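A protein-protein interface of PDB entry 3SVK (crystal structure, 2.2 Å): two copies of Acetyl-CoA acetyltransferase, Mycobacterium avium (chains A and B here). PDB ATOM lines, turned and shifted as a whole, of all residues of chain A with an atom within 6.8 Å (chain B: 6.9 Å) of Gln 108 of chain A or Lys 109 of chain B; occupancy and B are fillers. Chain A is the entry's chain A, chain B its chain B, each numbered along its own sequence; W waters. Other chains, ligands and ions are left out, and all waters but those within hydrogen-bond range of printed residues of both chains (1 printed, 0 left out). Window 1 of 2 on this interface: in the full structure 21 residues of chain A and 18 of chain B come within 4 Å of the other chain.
The side-chain amino group (NZ) of Lys 109 of chain B is in hydrogen-bond range of the side-chain amide oxygen (OE1) of Gln 108 of chain A, at 3.4 Å.
The side-chain amide nitrogen (NE2) of Gln 108 of chain A is in hydrogen-bond range of the side-chain hydroxyl (OG) of Ser 112 of chain B (3.1 Å).
The side-chain amide nitrogen of Gln 108 of chain A lies within hydrogen-bond range of the side-chain carboxylate of Asp 115 of chain B.
The side-chain amino group of Lys 109 of chain A sits at hydrogen-bond distance from the side-chain amide oxygen of Gln 108 of chain B, at 3.1 Å.
The guanidinium group (NH1) of Arg 111 of chain A is in hydrogen-bond range of the backbone carbonyl oxygen (O) of Ser 112 of chain B (3.0 Å).
The side-chain amide nitrogen (NE2) of Gln 108 of chain B lies within hydrogen-bond range of the side-chain hydroxyl (OG) of Ser 112 of chain A, at 3.2 Å.
O of Ser 112 of chain A is in hydrogen-bond range of NH1 of Arg 111 of chain B, 3.1 Å away.
The side-chain carboxylate (OD2) of Asp 115 of chain A sits at hydrogen-bond distance from the side-chain amide nitrogen (NE2) of Gln 108 of chain B (3.2 Å).
NH2 of Arg 317 of chain A sits at hydrogen-bond distance from O of Trp 114 of chain B, 3.0 Å away.
The side-chain carboxylate of Asp 115 of chain B lies within salt-bridge range of the guanidinium group of Arg 317 of chain A, at 3.0 Å.
The guanidinium group (NH1) of Arg 111 of chain A sits close to the indole nitrogen (NE1) of Trp 114 of chain B (3.3 Å).
The side-chain amide oxygen of Asn 104 of chain A sits close to the side-chain amide oxygen of Gln 108 of chain A (3.5 Å).
The backbone carbonyl oxygen of Thr 293 of chain A sits at hydrogen-bond distance from the guanidinium group of Arg 317 of chain A (2.7 Å).
OD1 of Asp 57 of chain B is in salt-bridge range of NZ of Lys 109 of chain B, 3.5 Å away.
The side-chain hydroxyl of Ser 112 of chain B sits at hydrogen-bond distance from the backbone carbonyl oxygen of Lys 109 of chain B (2.9 Å).
The side-chain amino group (NZ) of Lys 109 of chain B is in salt-bridge range of the side-chain carboxylate (OD2) of Asp 115 of chain B, 3.3 Å away.
The side-chain hydroxyl (OG) of Ser 112 of chain B lies close to the backbone NH (N) of Trp 114 of chain B, 3.4 Å away.
Among the printed residues, pairs that only touch across the chains: Gly 99 of chain A with Val 90 of chain B (3.96 Å), Leu 100 of chain A with Val 90 of chain B (3.9 Å), Gln 108 of chain A with Trp 114 of chain B (3.9 Å), Arg 111 of chain A with Arg 111 of chain B (3.8 Å), Ile 290 of chain A with Trp 114 of chain B (3.9 Å) and Thr 293 of chain A with Trp 114 of chain B (3.7 Å).
Ala 107 of chain A touches none of the printed residues of chain B.
Of chain B, only Lys 109, Ser 112, Trp 114 and Asp 115 come within 4 Å of Gln 108 of chain A.
Ile 59 of chain B touches none of the printed residues of chain A.
Printed residues of chain A within 4 Å of Gln 108 of chain B: Lys 109 (3.1 Å), Ser 112 (3.2 Å) and Asp 115 (3.2 Å).
Of chain A, only Gln 108 (3.4 Å) comes within 4 Å of Lys 109 of chain B.
Printed residues of chain A within 4 Å of Asp 115 of chain B: Gln 108 (3.2 Å) and Arg 317 (3.0 Å).
The nearest printed residue of chain B that does not touch Asp 115 of chain A is Asn 104 of chain B (7.2 Å).
Of the 18 printed residues of chain B, 7 touch a printed residue of chain A.
Hydrophobic or aromatic side chains of chain B that line the printed part of chain A: Val 90 and Trp 114.
Along chain B the printed residues that touch a printed residue of chain A span positions 90 to 115.
Hydrophobic or aromatic side chains of chain A that line the printed part of chain B: Leu 100.
Along chain A the printed residues that touch a printed residue of chain B span positions 99 to 317.
Among the printed residues, 17 pairs touch across the chains.
Gln 108 of chain A touches Lys 109 of chain B, and with the chains exchanged Lys 109 of chain A touches Gln 108 of chain B.
Gln 108 of chain A touches Asp 115 of chain B, and with the chains exchanged Asp 115 of chain A touches Gln 108 of chain B.
Arg 111 of chain B touches its own counterpart, Arg 111 of chain A.
Arg 111 of chain A touches Ser 112 of chain B, and with the chains exchanged Ser 112 of chain A touches Arg 111 of chain B.
Of the 17 pairs that touch across the chains among the printed residues, 9 have their exchanged pair printed and touching as well.
Water W1 bridges NE2 of Gln 108 of chain B (2.6 Å) and OD2 of Asp 115 of chain A (2.9 Å).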
ATOM      1  N   ALA A   9      24.585   4.245  -5.889  1.00  0.00           N
ATOM      2  CA  ALA A   9      25.540   4.623  -6.907  1.00  0.00           C
ATOM      3  C   ALA A   9      25.285   6.087  -7.230  1.00  0.00           C
ATOM      4  O   ALA A   9      24.153   6.469  -7.510  1.00  0.00           O
ATOM      5  CB  ALA A   9      25.422   3.722  -8.150  1.00  0.00           C
ATOM      6  N   GLY A  99      23.851  -7.133 -24.635  1.00  0.00           N
ATOM      7  CA  GLY A  99      22.783  -7.019 -23.618  1.00  0.00           C
ATOM      8  C   GLY A  99      23.129  -6.167 -22.392  1.00  0.00           C
ATOM      9  O   GLY A  99      22.360  -6.107 -21.422  1.00  0.00           O
ATOM     10  N   LEU A 100      24.285  -5.510 -22.428  1.00  0.00           N
ATOM     11  CA  LEU A 100      24.761  -4.713 -21.314  1.00  0.00           C
ATOM     12  C   LEU A 100      24.955  -3.282 -21.776  1.00  0.00           C
ATOM     13  O   LEU A 100      25.194  -3.028 -22.937  1.00  0.00           O
ATOM     14  CB  LEU A 100      26.088  -5.261 -20.793  1.00  0.00           C
ATOM     15  CG  LEU A 100      26.060  -6.700 -20.249  1.00  0.00           C
ATOM     16  CD1 LEU A 100      27.483  -7.173 -20.000  1.00  0.00           C
ATOM     17  CD2 LEU A 100      25.206  -6.785 -18.992  1.00  0.00           C
ATOM     18  N   VAL A 103      26.673   2.509 -18.466  1.00  0.00           N
ATOM     19  CA  VAL A 103      26.321   3.223 -17.245  1.00  0.00           C
ATOM     20  C   VAL A 103      25.581   2.329 -16.263  1.00  0.00           C
ATOM     21  O   VAL A 103      25.858   2.379 -15.064  1.00  0.00           O
ATOM     22  CB  VAL A 103      25.513   4.503 -17.557  1.00  0.00           C
ATOM     23  CG1 VAL A 103      25.012   5.129 -16.273  1.00  0.00           C
ATOM     24  CG2 VAL A 103      26.400   5.518 -18.370  1.00  0.00           C
ATOM     25  N   ASN A 104      24.664   1.512 -16.805  1.00  0.00           N
ATOM     26  CA  ASN A 104      23.878   0.492 -16.092  1.00  0.00           C
ATOM     27  C   ASN A 104      24.817  -0.549 -15.469  1.00  0.00           C
ATOM     28  O   ASN A 104      24.683  -0.876 -14.291  1.00  0.00           O
ATOM     29  CB  ASN A 104      22.875  -0.130 -17.101  1.00  0.00           C
ATOM     30  CG  ASN A 104      22.228  -1.427 -16.635  1.00  0.00           C
ATOM     31  OD1 ASN A 104      22.910  -2.379 -16.244  1.00  0.00           O
ATOM     32  ND2 ASN A 104      20.898  -1.503 -16.748  1.00  0.00           N
ATOM     33  N   THR A 105      25.788  -1.047 -16.239  1.00  0.00           N
ATOM     34  CA  THR A 105      26.790  -1.951 -15.677  1.00  0.00           C
ATOM     35  C   THR A 105      27.595  -1.292 -14.557  1.00  0.00           C
ATOM     36  O   THR A 105      27.978  -1.967 -13.609  1.00  0.00           O
ATOM     37  CB  THR A 105      27.807  -2.467 -16.738  1.00  0.00           C
ATOM     38  OG1 THR A 105      27.145  -3.283 -17.729  1.00  0.00           O
ATOM     39  CG2 THR A 105      28.923  -3.282 -16.060  1.00  0.00           C
ATOM     40  N   ALA A 106      27.879   0.005 -14.673  1.00  0.00           N
ATOM     41  CA  ALA A 106      28.724   0.678 -13.686  1.00  0.00           C
ATOM     42  C   ALA A 106      27.937   0.833 -12.386  1.00  0.00           C
ATOM     43  O   ALA A 106      28.458   0.609 -11.298  1.00  0.00           O
ATOM     44  CB  ALA A 106      29.208   2.083 -14.222  1.00  0.00           C
ATOM     45  N   ALA A 107      26.663   1.193 -12.521  1.00  0.00           N
ATOM     46  CA  ALA A 107      25.805   1.380 -11.375  1.00  0.00           C
ATOM     47  C   ALA A 107      25.731   0.107 -10.574  1.00  0.00           C
ATOM     48  O   ALA A 107      25.884   0.118  -9.349  1.00  0.00           O
ATOM     49  CB  ALA A 107      24.398   1.840 -11.812  1.00  0.00           C
ATOM     50  N   GLN A 108      25.524  -1.002 -11.268  1.00  0.00           N
ATOM     51  CA  GLN A 108      25.324  -2.274 -10.577  1.00  0.00           C
ATOM     52  C   GLN A 108      26.606  -2.703  -9.873  1.00  0.00           C
ATOM     53  O   GLN A 108      26.535  -3.181  -8.763  1.00  0.00           O
ATOM     54  CB  GLN A 108      24.775  -3.359 -11.528  1.00  0.00           C
ATOM     55  CG  GLN A 108      23.286  -3.116 -11.888  1.00  0.00           C
ATOM     56  CD  GLN A 108      22.656  -4.309 -12.575  1.00  0.00           C
ATOM     57  OE1 GLN A 108      23.082  -4.692 -13.657  1.00  0.00           O
ATOM     58  NE2 GLN A 108      21.657  -4.919 -11.937  1.00  0.00           N
ATOM     59  N   LYS A 109      27.764  -2.482 -10.498  1.00  0.00           N
ATOM     60  CA  LYS A 109      29.031  -2.780  -9.855  1.00  0.00           C
ATOM     61  C   LYS A 109      29.189  -1.992  -8.562  1.00  0.00           C
ATOM     62  O   LYS A 109      29.603  -2.532  -7.562  1.00  0.00           O
ATOM     63  CB  LYS A 109      30.216  -2.490 -10.760  1.00  0.00           C
ATOM     64  CG  LYS A 109      30.449  -3.454 -11.935  1.00  0.00           C
ATOM     65  CD  LYS A 109      31.703  -3.056 -12.749  1.00  0.00           C
ATOM     66  CE  LYS A 109      32.330  -4.232 -13.492  1.00  0.00           C
ATOM     67  NZ  LYS A 109      32.781  -5.320 -12.532  1.00  0.00           N
ATOM     68  N   VAL A 110      28.880  -0.709  -8.579  1.00  0.00           N
ATOM     69  CA  VAL A 110      29.039   0.111  -7.377  1.00  0.00           C
ATOM     70  C   VAL A 110      28.059  -0.337  -6.309  1.00  0.00           C
ATOM     71  O   VAL A 110      28.415  -0.529  -5.141  1.00  0.00           O
ATOM     72  CB  VAL A 110      28.831   1.605  -7.685  1.00  0.00           C
ATOM     73  CG1 VAL A 110      28.745   2.419  -6.386  1.00  0.00           C
ATOM     74  CG2 VAL A 110      29.950   2.102  -8.604  1.00  0.00           C
ATOM     75  N   ARG A 111      26.815  -0.496  -6.730  1.00  0.00           N
ATOM     76  CA  ARG A 111      25.746  -0.952  -5.862  1.00  0.00           C
ATOM     77  C   ARG A 111      26.038  -2.341  -5.282  1.00  0.00           C
ATOM     78  O   ARG A 111      25.581  -2.698  -4.184  1.00  0.00           O
ATOM     79  CB  ARG A 111      24.449  -1.018  -6.661  1.00  0.00           C
ATOM     80  CG  ARG A 111      23.531   0.191  -6.576  1.00  0.00           C
ATOM     81  CD  ARG A 111      22.127  -0.320  -6.245  1.00  0.00           C
ATOM     82  NE  ARG A 111      21.227   0.716  -5.742  1.00  0.00           N
ATOM     83  CZ  ARG A 111      19.992   0.488  -5.310  1.00  0.00           C
ATOM     84  NH1 ARG A 111      19.494  -0.746  -5.296  1.00  0.00           N
ATOM     85  NH2 ARG A 111      19.248   1.505  -4.877  1.00  0.00           N
ATOM     86  N   SER A 112      26.778  -3.143  -6.040  1.00  0.00           N
ATOM     87  CA  SER A 112      27.153  -4.462  -5.571  1.00  0.00           C
ATOM     88  C   SER A 112      28.049  -4.337  -4.334  1.00  0.00           C
ATOM     89  O   SER A 112      28.014  -5.204  -3.474  1.00  0.00           O
ATOM     90  CB  SER A 112      27.845  -5.264  -6.677  1.00  0.00           C
ATOM     91  OG  SER A 112      29.236  -5.299  -6.483  1.00  0.00           O
ATOM     92  N   GLY A 113      28.857  -3.276  -4.261  1.00  0.00           N
ATOM     93  CA  GLY A 113      29.611  -2.951  -3.051  1.00  0.00           C
ATOM     94  C   GLY A 113      31.103  -3.228  -3.090  1.00  0.00           C
ATOM     95  O   GLY A 113      31.848  -2.764  -2.229  1.00  0.00           O
ATOM     96  N   ASP A 115      33.156  -2.590  -5.917  1.00  0.00           N
ATOM     97  CA  ASP A 115      33.868  -1.553  -6.696  1.00  0.00           C
ATOM     98  C   ASP A 115      33.503  -0.139  -6.251  1.00  0.00           C
ATOM     99  O   ASP A 115      32.334   0.190  -6.076  1.00  0.00           O
ATOM    100  CB  ASP A 115      33.603  -1.696  -8.194  1.00  0.00           C
ATOM    101  CG  ASP A 115      34.005  -3.043  -8.727  1.00  0.00           C
ATOM    102  OD1 ASP A 115      35.194  -3.431  -8.581  1.00  0.00           O
ATOM    103  OD2 ASP A 115      33.116  -3.720  -9.282  1.00  0.00           O
ATOM    104  N   VAL A 273      31.234   7.122 -11.858  1.00  0.00           N
ATOM    105  CA  VAL A 273      30.243   6.601 -10.926  1.00  0.00           C
ATOM    106  C   VAL A 273      30.977   6.035  -9.701  1.00  0.00           C
ATOM    107  O   VAL A 273      32.039   5.388  -9.813  1.00  0.00           O
ATOM    108  CB  VAL A 273      29.382   5.485 -11.617  1.00  0.00           C
ATOM    109  CG1 VAL A 273      28.316   4.927 -10.674  1.00  0.00           C
ATOM    110  CG2 VAL A 273      28.730   6.003 -12.922  1.00  0.00           C
ATOM    111  N   ILE A 290      21.880   7.476  -8.861  1.00  0.00           N
ATOM    112  CA  ILE A 290      21.227   6.576  -9.796  1.00  0.00           C
ATOM    113  C   ILE A 290      20.174   5.790  -9.027  1.00  0.00           C
ATOM    114  O   ILE A 290      20.483   4.839  -8.306  1.00  0.00           O
ATOM    115  CB  ILE A 290      22.233   5.636 -10.520  1.00  0.00           C
ATOM    116  CG1 ILE A 290      23.229   6.457 -11.329  1.00  0.00           C
ATOM    117  CG2 ILE A 290      21.477   4.650 -11.405  1.00  0.00           C
ATOM    118  CD1 ILE A 290      24.357   5.617 -12.011  1.00  0.00           C
ATOM    119  N   THR A 293      17.680   1.353 -12.651  1.00  0.00           N
ATOM    120  CA  THR A 293      17.978   1.118 -14.034  1.00  0.00           C
ATOM    121  C   THR A 293      17.418  -0.247 -14.357  1.00  0.00           C
ATOM    122  O   THR A 293      17.366  -1.112 -13.507  1.00  0.00           O
ATOM    123  CB  THR A 293      19.467   1.110 -14.304  1.00  0.00           C
ATOM    124  OG1 THR A 293      19.685   1.265 -15.711  1.00  0.00           O
ATOM    125  CG2 THR A 293      20.052  -0.227 -13.872  1.00  0.00           C
ATOM    126  N   THR A 295      16.427  -3.016 -17.973  1.00  0.00           N
ATOM    127  CA  THR A 295      16.762  -3.421 -19.317  1.00  0.00           C
ATOM    128  C   THR A 295      15.600  -4.229 -19.874  1.00  0.00           C
ATOM    129  O   THR A 295      15.071  -5.124 -19.198  1.00  0.00           O
ATOM    130  CB  THR A 295      18.054  -4.320 -19.313  1.00  0.00           C
ATOM    131  OG1 THR A 295      19.225  -3.519 -19.577  1.00  0.00           O
ATOM    132  CG2 THR A 295      17.962  -5.383 -20.356  1.00  0.00           C
ATOM    133  N   ARG A 317      10.292  -0.280 -10.820  1.00  0.00           N
ATOM    134  CA  ARG A 317      11.335  -0.562  -9.831  1.00  0.00           C
ATOM    135  C   ARG A 317      11.554   0.578  -8.836  1.00  0.00           C
ATOM    136  O   ARG A 317      11.750   0.334  -7.647  1.00  0.00           O
ATOM    137  CB  ARG A 317      12.666  -0.872 -10.536  1.00  0.00           C
ATOM    138  CG  ARG A 317      12.799  -2.321 -10.969  1.00  0.00           C
ATOM    139  CD  ARG A 317      13.846  -2.466 -12.058  1.00  0.00           C
ATOM    140  NE  ARG A 317      14.045  -3.866 -12.414  1.00  0.00           N
ATOM    141  CZ  ARG A 317      15.121  -4.347 -13.033  1.00  0.00           C
ATOM    142  NH1 ARG A 317      16.130  -3.552 -13.368  1.00  0.00           N
ATOM    143  NH2 ARG A 317      15.197  -5.645 -13.300  1.00  0.00           N
ATOM    144  N   SER B  56      15.356 -12.400 -14.424  1.00  0.00           N
ATOM    145  CA  SER B  56      15.582 -11.177 -15.197  1.00  0.00           C
ATOM    146  C   SER B  56      16.536 -11.345 -16.419  1.00  0.00           C
ATOM    147  O   SER B  56      16.466 -10.594 -17.401  1.00  0.00           O
ATOM    148  CB  SER B  56      16.202 -10.169 -14.256  1.00  0.00           C
ATOM    149  OG  SER B  56      17.499 -10.601 -13.895  1.00  0.00           O
ATOM    150  N   ASP B  57      17.450 -12.311 -16.339  1.00  0.00           N
ATOM    151  CA  ASP B  57      18.423 -12.517 -17.414  1.00  0.00           C
ATOM    152  C   ASP B  57      18.907 -13.942 -17.452  1.00  0.00           C
ATOM    153  O   ASP B  57      19.067 -14.575 -16.411  1.00  0.00           O
ATOM    154  CB  ASP B  57      19.666 -11.639 -17.214  1.00  0.00           C
ATOM    155  CG  ASP B  57      19.340 -10.162 -17.104  1.00  0.00           C
ATOM    156  OD1 ASP B  57      19.195  -9.673 -15.952  1.00  0.00           O
ATOM    157  OD2 ASP B  57      19.237  -9.504 -18.159  1.00  0.00           O
ATOM    158  N   ILE B  59      22.366 -15.408 -18.700  1.00  0.00           N
ATOM    159  CA  ILE B  59      23.695 -14.922 -19.053  1.00  0.00           C
ATOM    160  C   ILE B  59      24.521 -16.083 -19.570  1.00  0.00           C
ATOM    161  O   ILE B  59      24.787 -17.055 -18.853  1.00  0.00           O
ATOM    162  CB  ILE B  59      24.405 -14.272 -17.819  1.00  0.00           C
ATOM    163  CG1 ILE B  59      23.484 -13.210 -17.211  1.00  0.00           C
ATOM    164  CG2 ILE B  59      25.799 -13.696 -18.214  1.00  0.00           C
ATOM    165  CD1 ILE B  59      24.122 -12.357 -16.161  1.00  0.00           C
ATOM    166  N   VAL B  90      22.030 -12.047 -22.008  1.00  0.00           N
ATOM    167  CA  VAL B  90      23.358 -11.417 -22.045  1.00  0.00           C
ATOM    168  C   VAL B  90      24.374 -12.438 -22.565  1.00  0.00           C
ATOM    169  O   VAL B  90      24.482 -13.534 -22.019  1.00  0.00           O
ATOM    170  CB  VAL B  90      23.782 -10.916 -20.623  1.00  0.00           C
ATOM    171  CG1 VAL B  90      25.263 -10.455 -20.579  1.00  0.00           C
ATOM    172  CG2 VAL B  90      22.839  -9.831 -20.151  1.00  0.00           C
ATOM    173  N   ASN B 104      30.188 -14.079 -12.079  1.00  0.00           N
ATOM    174  CA  ASN B 104      30.574 -12.787 -11.523  1.00  0.00           C
ATOM    175  C   ASN B 104      29.531 -11.714 -11.907  1.00  0.00           C
ATOM    176  O   ASN B 104      29.108 -10.907 -11.068  1.00  0.00           O
ATOM    177  CB  ASN B 104      31.988 -12.457 -12.058  1.00  0.00           C
ATOM    178  CG  ASN B 104      32.423 -11.014 -11.804  1.00  0.00           C
ATOM    179  OD1 ASN B 104      33.255 -10.743 -10.947  1.00  0.00           O
ATOM    180  ND2 ASN B 104      31.885 -10.095 -12.583  1.00  0.00           N
ATOM    181  N   THR B 105      29.089 -11.711 -13.165  1.00  0.00           N
ATOM    182  CA  THR B 105      28.077 -10.734 -13.575  1.00  0.00           C
ATOM    183  C   THR B 105      26.743 -10.953 -12.883  1.00  0.00           C
ATOM    184  O   THR B 105      26.089  -9.980 -12.512  1.00  0.00           O
ATOM    185  CB  THR B 105      27.866 -10.694 -15.101  1.00  0.00           C
ATOM    186  OG1 THR B 105      29.099 -10.307 -15.714  1.00  0.00           O
ATOM    187  CG2 THR B 105      26.777  -9.670 -15.494  1.00  0.00           C
ATOM    188  N   ALA B 106      26.352 -12.210 -12.699  1.00  0.00           N
ATOM    189  CA  ALA B 106      25.050 -12.531 -12.117  1.00  0.00           C
ATOM    190  C   ALA B 106      25.018 -12.163 -10.647  1.00  0.00           C
ATOM    191  O   ALA B 106      24.011 -11.744 -10.140  1.00  0.00           O
ATOM    192  CB  ALA B 106      24.737 -14.037 -12.297  1.00  0.00           C
ATOM    193  N   ALA B 107      26.130 -12.348  -9.954  1.00  0.00           N
ATOM    194  CA  ALA B 107      26.205 -12.003  -8.550  1.00  0.00           C
ATOM    195  C   ALA B 107      26.101 -10.482  -8.379  1.00  0.00           C
ATOM    196  O   ALA B 107      25.420 -10.001  -7.477  1.00  0.00           O
ATOM    197  CB  ALA B 107      27.490 -12.530  -7.951  1.00  0.00           C
ATOM    198  N   GLN B 108      26.776  -9.734  -9.236  1.00  0.00           N
ATOM    199  CA  GLN B 108      26.740  -8.260  -9.129  1.00  0.00           C
ATOM    200  C   GLN B 108      25.332  -7.695  -9.407  1.00  0.00           C
ATOM    201  O   GLN B 108      24.863  -6.843  -8.652  1.00  0.00           O
ATOM    202  CB  GLN B 108      27.846  -7.597  -9.988  1.00  0.00           C
ATOM    203  CG  GLN B 108      29.215  -7.728  -9.279  1.00  0.00           C
ATOM    204  CD  GLN B 108      30.319  -6.907  -9.912  1.00  0.00           C
ATOM    205  OE1 GLN B 108      30.703  -7.142 -11.051  1.00  0.00           O
ATOM    206  NE2 GLN B 108      30.847  -5.958  -9.163  1.00  0.00           N
ATOM    207  N   LYS B 109      24.661  -8.245 -10.432  1.00  0.00           N
ATOM    208  CA  LYS B 109      23.277  -7.923 -10.718  1.00  0.00           C
ATOM    209  C   LYS B 109      22.415  -8.148  -9.486  1.00  0.00           C
ATOM    210  O   LYS B 109      21.690  -7.255  -9.073  1.00  0.00           O
ATOM    211  CB  LYS B 109      22.737  -8.754 -11.875  1.00  0.00           C
ATOM    212  CG  LYS B 109      23.215  -8.328 -13.299  1.00  0.00           C
ATOM    213  CD  LYS B 109      22.476  -9.106 -14.421  1.00  0.00           C
ATOM    214  CE  LYS B 109      22.404  -8.308 -15.669  1.00  0.00           C
ATOM    215  NZ  LYS B 109      21.551  -7.090 -15.483  1.00  0.00           N
ATOM    216  N   VAL B 110      22.497  -9.331  -8.904  1.00  0.00           N
ATOM    217  CA  VAL B 110      21.688  -9.670  -7.716  1.00  0.00           C
ATOM    218  C   VAL B 110      22.072  -8.858  -6.481  1.00  0.00           C
ATOM    219  O   VAL B 110      21.224  -8.405  -5.744  1.00  0.00           O
ATOM    220  CB  VAL B 110      21.802 -11.175  -7.380  1.00  0.00           C
ATOM    221  CG1 VAL B 110      21.217 -11.472  -5.969  1.00  0.00           C
ATOM    222  CG2 VAL B 110      21.124 -11.994  -8.484  1.00  0.00           C
ATOM    223  N   ARG B 111      23.361  -8.683  -6.254  1.00  0.00           N
ATOM    224  CA  ARG B 111      23.835  -7.861  -5.141  1.00  0.00           C
ATOM    225  C   ARG B 111      23.413  -6.416  -5.261  1.00  0.00           C
ATOM    226  O   ARG B 111      23.267  -5.709  -4.246  1.00  0.00           O
ATOM    227  CB  ARG B 111      25.360  -7.879  -5.067  1.00  0.00           C
ATOM    228  CG  ARG B 111      25.981  -8.923  -4.152  1.00  0.00           C
ATOM    229  CD  ARG B 111      27.028  -8.202  -3.306  1.00  0.00           C
ATOM    230  NE  ARG B 111      27.314  -8.882  -2.047  1.00  0.00           N
ATOM    231  CZ  ARG B 111      28.115  -8.401  -1.103  1.00  0.00           C
ATOM    232  NH1 ARG B 111      28.722  -7.215  -1.256  1.00  0.00           N
ATOM    233  NH2 ARG B 111      28.315  -9.122   0.002  1.00  0.00           N
ATOM    234  N   SER B 112      23.269  -5.952  -6.502  1.00  0.00           N
ATOM    235  CA  SER B 112      22.840  -4.586  -6.745  1.00  0.00           C
ATOM    236  C   SER B 112      21.397  -4.385  -6.287  1.00  0.00           C
ATOM    237  O   SER B 112      20.977  -3.250  -6.049  1.00  0.00           O
ATOM    238  CB  SER B 112      22.972  -4.217  -8.220  1.00  0.00           C
ATOM    239  OG  SER B 112      21.730  -4.348  -8.878  1.00  0.00           O
ATOM    240  N   GLY B 113      20.633  -5.476  -6.199  1.00  0.00           N
ATOM    241  CA  GLY B 113      19.284  -5.440  -5.617  1.00  0.00           C
ATOM    242  C   GLY B 113      18.151  -5.144  -6.589  1.00  0.00           C
ATOM    243  O   GLY B 113      16.982  -5.151  -6.198  1.00  0.00           O
ATOM    244  N   TRP B 114      18.485  -4.881  -7.852  1.00  0.00           N
ATOM    245  CA  TRP B 114      17.471  -4.626  -8.876  1.00  0.00           C
ATOM    246  C   TRP B 114      17.085  -5.849  -9.704  1.00  0.00           C
ATOM    247  O   TRP B 114      16.135  -5.755 -10.473  1.00  0.00           O
ATOM    248  CB  TRP B 114      17.923  -3.523  -9.835  1.00  0.00           C
ATOM    249  CG  TRP B 114      18.049  -2.185  -9.231  1.00  0.00           C
ATOM    250  CD1 TRP B 114      17.192  -1.594  -8.344  1.00  0.00           C
ATOM    251  CD2 TRP B 114      19.082  -1.233  -9.488  1.00  0.00           C
ATOM    252  NE1 TRP B 114      17.646  -0.343  -8.021  1.00  0.00           N
ATOM    253  CE2 TRP B 114      18.805  -0.098  -8.706  1.00  0.00           C
ATOM    254  CE3 TRP B 114      20.224  -1.235 -10.294  1.00  0.00           C
ATOM    255  CZ2 TRP B 114      19.628   1.030  -8.709  1.00  0.00           C
ATOM    256  CZ3 TRP B 114      21.040  -0.111 -10.306  1.00  0.00           C
ATOM    257  CH2 TRP B 114      20.737   1.007  -9.514  1.00  0.00           C
ATOM    258  N   ASP B 115      17.812  -6.967  -9.585  1.00  0.00           N
ATOM    259  CA  ASP B 115      17.424  -8.240 -10.221  1.00  0.00           C
ATOM    260  C   ASP B 115      17.275  -9.333  -9.168  1.00  0.00           C
ATOM    261  O   ASP B 115      18.080  -9.418  -8.235  1.00  0.00           O
ATOM    262  CB  ASP B 115      18.479  -8.711 -11.242  1.00  0.00           C
ATOM    263  CG  ASP B 115      18.625  -7.777 -12.416  1.00  0.00           C
ATOM    264  OD1 ASP B 115      17.606  -7.462 -13.067  1.00  0.00           O
ATOM    265  OD2 ASP B 115      19.770  -7.360 -12.692  1.00  0.00           O
ATOM    266  N   ASP B 116      16.281 -10.202  -9.345  1.00  0.00           N
ATOM    267  CA  ASP B 116      15.883 -11.140  -8.287  1.00  0.00           C
ATOM    268  C   ASP B 116      16.448 -12.553  -8.479  1.00  0.00           C
ATOM    269  O   ASP B 116      16.917 -13.182  -7.512  1.00  0.00           O
ATOM    270  CB  ASP B 116      14.350 -11.187  -8.186  1.00  0.00           C
ATOM    271  CG  ASP B 116      13.735  -9.858  -7.720  1.00  0.00           C
ATOM    272  OD1 ASP B 116      14.035  -9.392  -6.595  1.00  0.00           O
ATOM    273  OD2 ASP B 116      12.911  -9.301  -8.467  1.00  0.00           O
ATOM    274  N   VAL B 118      18.827 -14.833 -11.528  1.00  0.00           N
ATOM    275  CA  VAL B 118      19.544 -14.833 -12.800  1.00  0.00           C
ATOM    276  C   VAL B 118      19.986 -16.261 -13.085  1.00  0.00           C
ATOM    277  O   VAL B 118      20.340 -16.965 -12.164  1.00  0.00           O
ATOM    278  CB  VAL B 118      20.791 -13.891 -12.765  1.00  0.00           C
ATOM    279  CG1 VAL B 118      21.428 -13.798 -14.176  1.00  0.00           C
ATOM    280  CG2 VAL B 118      20.403 -12.483 -12.245  1.00  0.00           C
HETATM  281  O   HOH W   1      33.264  -6.524  -8.494  1.00  0.00           O
